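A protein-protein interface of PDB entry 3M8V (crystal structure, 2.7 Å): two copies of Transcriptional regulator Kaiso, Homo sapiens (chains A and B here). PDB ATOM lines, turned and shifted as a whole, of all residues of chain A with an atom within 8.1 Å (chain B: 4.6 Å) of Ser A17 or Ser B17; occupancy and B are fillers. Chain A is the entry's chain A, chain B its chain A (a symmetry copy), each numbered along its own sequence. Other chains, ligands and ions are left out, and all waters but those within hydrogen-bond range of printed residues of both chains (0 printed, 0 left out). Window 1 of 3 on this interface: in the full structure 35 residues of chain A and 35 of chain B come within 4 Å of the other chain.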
ATOM      1  N   THR A  12      35.203   5.073  29.096  1.00  0.00           N
ATOM      2  CA  THR A  12      34.728   6.422  28.829  1.00  0.00           C
ATOM      3  C   THR A  12      33.331   6.386  28.221  1.00  0.00           C
ATOM      4  O   THR A  12      33.066   5.622  27.284  1.00  0.00           O
ATOM      5  CB  THR A  12      35.671   7.155  27.873  1.00  0.00           C
ATOM      6  OG1 THR A  12      36.972   7.247  28.465  1.00  0.00           O
ATOM      7  CG2 THR A  12      35.163   8.540  27.599  1.00  0.00           C
ATOM      8  N   ASP A  13      32.438   7.209  28.759  1.00  0.00           N
ATOM      9  CA  ASP A  13      31.084   7.309  28.235  1.00  0.00           C
ATOM     10  C   ASP A  13      31.031   8.462  27.234  1.00  0.00           C
ATOM     11  O   ASP A  13      30.864   9.621  27.602  1.00  0.00           O
ATOM     12  CB  ASP A  13      30.072   7.485  29.381  1.00  0.00           C
ATOM     13  CG  ASP A  13      28.612   7.536  28.904  1.00  0.00           C
ATOM     14  OD1 ASP A  13      28.326   7.250  27.722  1.00  0.00           O
ATOM     15  OD2 ASP A  13      27.733   7.855  29.733  1.00  0.00           O
ATOM     16  N   ILE A  14      31.183   8.119  25.961  1.00  0.00           N
ATOM     17  CA  ILE A  14      31.190   9.088  24.870  1.00  0.00           C
ATOM     18  C   ILE A  14      29.939   9.958  24.831  1.00  0.00           C
ATOM     19  O   ILE A  14      29.989  11.119  24.425  1.00  0.00           O
ATOM     20  CB  ILE A  14      31.350   8.384  23.498  1.00  0.00           C
ATOM     21  CG1 ILE A  14      32.821   8.285  23.105  1.00  0.00           C
ATOM     22  CG2 ILE A  14      30.640   9.161  22.411  1.00  0.00           C
ATOM     23  CD1 ILE A  14      33.766   8.336  24.271  1.00  0.00           C
ATOM     24  N   GLN A  15      28.811   9.400  25.243  1.00  0.00           N
ATOM     25  CA  GLN A  15      27.567  10.151  25.181  1.00  0.00           C
ATOM     26  C   GLN A  15      27.245  10.929  26.466  1.00  0.00           C
ATOM     27  O   GLN A  15      26.247  11.641  26.532  1.00  0.00           O
ATOM     28  CB  GLN A  15      26.397   9.251  24.740  1.00  0.00           C
ATOM     29  CG  GLN A  15      26.373   7.857  25.336  1.00  0.00           C
ATOM     30  CD  GLN A  15      25.386   6.927  24.624  1.00  0.00           C
ATOM     31  OE1 GLN A  15      24.841   7.272  23.576  1.00  0.00           O
ATOM     32  NE2 GLN A  15      25.155   5.744  25.199  1.00  0.00           N
ATOM     33  N   TYR A  16      28.102  10.821  27.475  1.00  0.00           N
ATOM     34  CA  TYR A  16      27.771  11.392  28.775  1.00  0.00           C
ATOM     35  C   TYR A  16      27.496  12.883  28.702  1.00  0.00           C
ATOM     36  O   TYR A  16      26.419  13.353  29.066  1.00  0.00           O
ATOM     37  CB  TYR A  16      28.879  11.135  29.783  1.00  0.00           C
ATOM     38  CG  TYR A  16      28.527  11.626  31.152  1.00  0.00           C
ATOM     39  CD1 TYR A  16      27.537  11.000  31.886  1.00  0.00           C
ATOM     40  CD2 TYR A  16      29.173  12.715  31.713  1.00  0.00           C
ATOM     41  CE1 TYR A  16      27.195  11.441  33.151  1.00  0.00           C
ATOM     42  CE2 TYR A  16      28.841  13.168  32.985  1.00  0.00           C
ATOM     43  CZ  TYR A  16      27.850  12.523  33.700  1.00  0.00           C
ATOM     44  OH  TYR A  16      27.505  12.936  34.962  1.00  0.00           O
ATOM     45  N   SER A  17      28.490  13.617  28.229  1.00  0.00           N
ATOM     46  CA  SER A  17      28.418  15.069  28.113  1.00  0.00           C
ATOM     47  C   SER A  17      27.116  15.584  27.483  1.00  0.00           C
ATOM     48  O   SER A  17      26.457  16.462  28.035  1.00  0.00           O
ATOM     49  CB  SER A  17      29.631  15.557  27.331  1.00  0.00           C
ATOM     50  OG  SER A  17      30.835  15.107  27.955  1.00  0.00           O
ATOM     51  N   GLY A  18      26.738  15.039  26.334  1.00  0.00           N
ATOM     52  CA  GLY A  18      25.482  15.408  25.695  1.00  0.00           C
ATOM     53  C   GLY A  18      24.219  15.169  26.513  1.00  0.00           C
ATOM     54  O   GLY A  18      23.307  15.996  26.520  1.00  0.00           O
ATOM     55  N   SER A  19      24.141  14.031  27.192  1.00  0.00           N
ATOM     56  CA  SER A  19      22.948  13.701  27.963  1.00  0.00           C
ATOM     57  C   SER A  19      22.878  14.583  29.196  1.00  0.00           C
ATOM     58  O   SER A  19      21.823  15.114  29.528  1.00  0.00           O
ATOM     59  CB  SER A  19      22.954  12.220  28.363  1.00  0.00           C
ATOM     60  OG  SER A  19      22.000  11.954  29.389  1.00  0.00           O
ATOM     61  N   LEU A  20      24.013  14.727  29.876  1.00  0.00           N
ATOM     62  CA  LEU A  20      24.097  15.627  31.018  1.00  0.00           C
ATOM     63  C   LEU A  20      23.589  17.021  30.672  1.00  0.00           C
ATOM     64  O   LEU A  20      22.670  17.534  31.299  1.00  0.00           O
ATOM     65  CB  LEU A  20      25.532  15.738  31.523  1.00  0.00           C
ATOM     66  CG  LEU A  20      25.634  16.630  32.759  1.00  0.00           C
ATOM     67  CD1 LEU A  20      24.677  16.144  33.834  1.00  0.00           C
ATOM     68  CD2 LEU A  20      27.027  16.631  33.288  1.00  0.00           C
ATOM     69  N   LEU A  21      24.218  17.632  29.675  1.00  0.00           N
ATOM     70  CA  LEU A  21      23.863  18.973  29.235  1.00  0.00           C
ATOM     71  C   LEU A  21      22.399  19.090  28.892  1.00  0.00           C
ATOM     72  O   LEU A  21      21.754  20.066  29.252  1.00  0.00           O
ATOM     73  CB  LEU A  21      24.681  19.359  28.019  1.00  0.00           C
ATOM     74  CG  LEU A  21      26.066  19.901  28.328  1.00  0.00           C
ATOM     75  CD1 LEU A  21      26.779  20.196  27.017  1.00  0.00           C
ATOM     76  CD2 LEU A  21      25.970  21.145  29.204  1.00  0.00           C
ATOM     77  N   ASN A  22      21.885  18.099  28.174  1.00  0.00           N
ATOM     78  CA  ASN A  22      20.476  18.083  27.803  1.00  0.00           C
ATOM     79  C   ASN A  22      19.547  17.974  29.013  1.00  0.00           C
ATOM     80  O   ASN A  22      18.532  18.660  29.092  1.00  0.00           O
ATOM     81  CB  ASN A  22      20.176  16.973  26.788  1.00  0.00           C
ATOM     82  CG  ASN A  22      18.699  16.917  26.427  1.00  0.00           C
ATOM     83  OD1 ASN A  22      18.220  17.759  25.668  1.00  0.00           O
ATOM     84  ND2 ASN A  22      17.958  15.947  26.999  1.00  0.00           N
ATOM     85  N   SER A  23      19.890  17.118  29.965  1.00  0.00           N
ATOM     86  CA  SER A  23      19.119  17.070  31.199  1.00  0.00           C
ATOM     87  C   SER A  23      19.177  18.434  31.909  1.00  0.00           C
ATOM     88  O   SER A  23      18.181  18.892  32.468  1.00  0.00           O
ATOM     89  CB  SER A  23      19.579  15.923  32.113  1.00  0.00           C
ATOM     90  OG  SER A  23      19.404  14.657  31.488  1.00  0.00           O
ATOM     91  N   LEU A  24      20.338  19.088  31.863  1.00  0.00           N
ATOM     92  CA  LEU A  24      20.529  20.364  32.550  1.00  0.00           C
ATOM     93  C   LEU A  24      19.718  21.473  31.878  1.00  0.00           C
ATOM     94  O   LEU A  24      19.165  22.357  32.540  1.00  0.00           O
ATOM     95  CB  LEU A  24      22.012  20.736  32.591  1.00  0.00           C
ATOM     96  CG  LEU A  24      22.925  19.977  33.552  1.00  0.00           C
ATOM     97  CD1 LEU A  24      24.382  20.260  33.224  1.00  0.00           C
ATOM     98  CD2 LEU A  24      22.624  20.368  34.973  1.00  0.00           C
ATOM     99  N   TYR A  86      24.051  27.957  24.186  1.00  0.00           N
ATOM    100  CA  TYR A  86      25.397  27.438  24.027  1.00  0.00           C
ATOM    101  C   TYR A  86      25.881  26.911  25.354  1.00  0.00           C
ATOM    102  O   TYR A  86      26.317  25.757  25.476  1.00  0.00           O
ATOM    103  CB  TYR A  86      26.369  28.510  23.528  1.00  0.00           C
ATOM    104  CG  TYR A  86      27.811  28.159  23.823  1.00  0.00           C
ATOM    105  CD1 TYR A  86      28.509  27.274  23.007  1.00  0.00           C
ATOM    106  CD2 TYR A  86      28.477  28.693  24.925  1.00  0.00           C
ATOM    107  CE1 TYR A  86      29.827  26.938  23.273  1.00  0.00           C
ATOM    108  CE2 TYR A  86      29.798  28.361  25.200  1.00  0.00           C
ATOM    109  CZ  TYR A  86      30.466  27.480  24.372  1.00  0.00           C
ATOM    110  OH  TYR A  86      31.773  27.134  24.638  1.00  0.00           O
ATOM    111  N   ILE A  87      25.807  27.763  26.362  1.00  0.00           N
ATOM    112  CA  ILE A  87      26.233  27.346  27.684  1.00  0.00           C
ATOM    113  C   ILE A  87      25.610  25.998  28.058  1.00  0.00           C
ATOM    114  O   ILE A  87      26.228  25.198  28.744  1.00  0.00           O
ATOM    115  CB  ILE A  87      25.970  28.436  28.735  1.00  0.00           C
ATOM    116  CG1 ILE A  87      27.056  29.504  28.619  1.00  0.00           C
ATOM    117  CG2 ILE A  87      25.990  27.846  30.130  1.00  0.00           C
ATOM    118  CD1 ILE A  87      26.859  30.701  29.497  1.00  0.00           C
ATOM    119  N   TYR A  88      24.406  25.737  27.565  1.00  0.00           N
ATOM    120  CA  TYR A  88      23.717  24.490  27.866  1.00  0.00           C
ATOM    121  C   TYR A  88      23.729  23.438  26.746  1.00  0.00           C
ATOM    122  O   TYR A  88      23.005  22.451  26.820  1.00  0.00           O
ATOM    123  CB  TYR A  88      22.279  24.778  28.308  1.00  0.00           C
ATOM    124  CG  TYR A  88      22.182  25.262  29.733  1.00  0.00           C
ATOM    125  CD1 TYR A  88      22.144  26.613  30.029  1.00  0.00           C
ATOM    126  CD2 TYR A  88      22.152  24.358  30.790  1.00  0.00           C
ATOM    127  CE1 TYR A  88      22.063  27.054  31.346  1.00  0.00           C
ATOM    128  CE2 TYR A  88      22.078  24.783  32.095  1.00  0.00           C
ATOM    129  CZ  TYR A  88      22.036  26.128  32.372  1.00  0.00           C
ATOM    130  OH  TYR A  88      21.963  26.546  33.684  1.00  0.00           O
ATOM    131  N   SER A  89      24.550  23.621  25.718  1.00  0.00           N
ATOM    132  CA  SER A  89      24.607  22.610  24.657  1.00  0.00           C
ATOM    133  C   SER A  89      25.973  22.466  24.024  1.00  0.00           C
ATOM    134  O   SER A  89      26.265  21.451  23.411  1.00  0.00           O
ATOM    135  CB  SER A  89      23.580  22.894  23.560  1.00  0.00           C
ATOM    136  OG  SER A  89      23.988  23.993  22.762  1.00  0.00           O
ATOM    137  N   SER A  90      26.805  23.488  24.174  1.00  0.00           N
ATOM    138  CA  SER A  90      28.110  23.543  23.512  1.00  0.00           C
ATOM    139  C   SER A  90      27.990  23.959  22.048  1.00  0.00           C
ATOM    140  O   SER A  90      28.981  23.964  21.333  1.00  0.00           O
ATOM    141  CB  SER A  90      28.857  22.207  23.621  1.00  0.00           C
ATOM    142  OG  SER A  90      28.487  21.310  22.588  1.00  0.00           O
ATOM    143  N   GLN B  15      35.435  20.934  22.713  1.00  0.00           N
ATOM    144  CA  GLN B  15      36.054  20.815  24.024  1.00  0.00           C
ATOM    145  C   GLN B  15      35.153  21.276  25.180  1.00  0.00           C
ATOM    146  O   GLN B  15      35.536  21.186  26.344  1.00  0.00           O
ATOM    147  CB  GLN B  15      37.431  21.508  24.052  1.00  0.00           C
ATOM    148  CG  GLN B  15      37.521  22.834  23.324  1.00  0.00           C
ATOM    149  CD  GLN B  15      38.965  23.301  23.123  1.00  0.00           C
ATOM    150  OE1 GLN B  15      39.909  22.552  23.374  1.00  0.00           O
ATOM    151  NE2 GLN B  15      39.136  24.545  22.668  1.00  0.00           N
ATOM    152  N   TYR B  16      33.948  21.737  24.869  1.00  0.00           N
ATOM    153  CA  TYR B  16      33.113  22.346  25.897  1.00  0.00           C
ATOM    154  C   TYR B  16      32.843  21.407  27.058  1.00  0.00           C
ATOM    155  O   TYR B  16      33.162  21.704  28.208  1.00  0.00           O
ATOM    156  CB  TYR B  16      31.790  22.820  25.317  1.00  0.00           C
ATOM    157  CG  TYR B  16      30.951  23.536  26.328  1.00  0.00           C
ATOM    158  CD1 TYR B  16      31.335  24.776  26.804  1.00  0.00           C
ATOM    159  CD2 TYR B  16      29.780  22.977  26.814  1.00  0.00           C
ATOM    160  CE1 TYR B  16      30.575  25.451  27.741  1.00  0.00           C
ATOM    161  CE2 TYR B  16      29.005  23.647  27.755  1.00  0.00           C
ATOM    162  CZ  TYR B  16      29.408  24.886  28.213  1.00  0.00           C
ATOM    163  OH  TYR B  16      28.662  25.579  29.132  1.00  0.00           O
ATOM    164  N   SER B  17      32.247  20.271  26.738  1.00  0.00           N
ATOM    165  CA  SER B  17      31.883  19.259  27.723  1.00  0.00           C
ATOM    166  C   SER B  17      32.997  18.934  28.728  1.00  0.00           C
ATOM    167  O   SER B  17      32.775  18.949  29.937  1.00  0.00           O
ATOM    168  CB  SER B  17      31.428  18.003  26.990  1.00  0.00           C
ATOM    169  OG  SER B  17      30.362  18.315  26.092  1.00  0.00           O
ATOM    170  N   GLY B  18      34.196  18.649  28.238  1.00  0.00           N
ATOM    171  CA  GLY B  18      35.334  18.398  29.112  1.00  0.00           C
ATOM    172  C   GLY B  18      35.715  19.532  30.058  1.00  0.00           C
ATOM    173  O   GLY B  18      36.041  19.299  31.222  1.00  0.00           O
ATOM    174  N   SER B  19      35.698  20.765  29.566  1.00  0.00           N
ATOM    175  CA  SER B  19      36.094  21.902  30.388  1.00  0.00           C
ATOM    176  C   SER B  19      35.025  22.174  31.430  1.00  0.00           C
ATOM    177  O   SER B  19      35.330  22.402  32.596  1.00  0.00           O
ATOM    178  CB  SER B  19      36.323  23.145  29.518  1.00  0.00           C
ATOM    179  OG  SER B  19      36.368  24.332  30.308  1.00  0.00           O
ATOM    180  N   LEU B  20      33.768  22.154  30.995  1.00  0.00           N
ATOM    181  CA  LEU B  20      32.650  22.300  31.917  1.00  0.00           C
ATOM    182  C   LEU B  20      32.749  21.320  33.079  1.00  0.00           C
ATOM    183  O   LEU B  20      32.774  21.713  34.239  1.00  0.00           O
ATOM    184  CB  LEU B  20      31.319  22.083  31.204  1.00  0.00           C
ATOM    185  CG  LEU B  20      30.130  22.293  32.140  1.00  0.00           C
ATOM    186  CD1 LEU B  20      30.218  23.658  32.799  1.00  0.00           C
ATOM    187  CD2 LEU B  20      28.848  22.179  31.388  1.00  0.00           C
ATOM    188  N   LEU B  21      32.786  20.035  32.747  1.00  0.00           N
ATOM    189  CA  LEU B  21      32.863  18.975  33.741  1.00  0.00           C
ATOM    190  C   LEU B  21      34.029  19.160  34.679  1.00  0.00           C
ATOM    191  O   LEU B  21      33.892  18.976  35.882  1.00  0.00           O
ATOM    192  CB  LEU B  21      32.995  17.627  33.060  1.00  0.00           C
ATOM    193  CG  LEU B  21      31.683  17.011  32.605  1.00  0.00           C
ATOM    194  CD1 LEU B  21      31.979  15.695  31.902  1.00  0.00           C
ATOM    195  CD2 LEU B  21      30.747  16.813  33.791  1.00  0.00           C
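Ile A14 touches none of the printed residues of chain B. Ser A17 touches just one residue of chain B: Ser B17. Of the printed residues of chain B, Leu A20 touches Leu B21 (3.8 Å). Ser A23 touches none of the printed residues of chain B. Printed residues of chain B within 4 Å of Tyr A86: Tyr B16. Of the printed residues of chain A, Ser B17 touches Ser A17. No residue of chain A comes within 4 Å of Gly B18. Of the printed residues of chain A, Leu B20 touches Leu A21.
Ser B17 touches its own counterpart, Ser A17. Leu A20 touches Leu B21, and with the chains exchanged Leu A21 touches Leu B20. Positions printed for both chains: 15, 16, 17, 18, 19, 20 and 21. Of the 6 pairs that touch across the chains among the printed residues, 3 have their exchanged pair printed and touching as well.
Of the 18 printed residues of chain A, 6 touch a printed residue of chain B. Hydrophobic or aromatic side chains of chain A within 4 Å of the printed part of chain B: Leu A20, Leu A21, Tyr A86 and Ile A87. Among the printed residues, no Asp or Glu carboxylate lies within 4 Å of a Lys or Arg side-chain nitrogen of the other chain.
Among the printed residues, pairs that only touch across the chains: Ser A17 with Ser B17 (3.1 Å), Leu A20 with Leu B21 (3.8 Å), Leu A21 with Leu B20 (3.8 Å), Tyr A86 with Tyr B16 (3.2 Å) and Ser A90 with Tyr B16 (3.4 Å).
The backbone carbonyl oxygen (O) of Ile A87 sits at hydrogen-bond distance from the side-chain hydroxyl (OH) of Tyr B16, 2.5 Å away.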
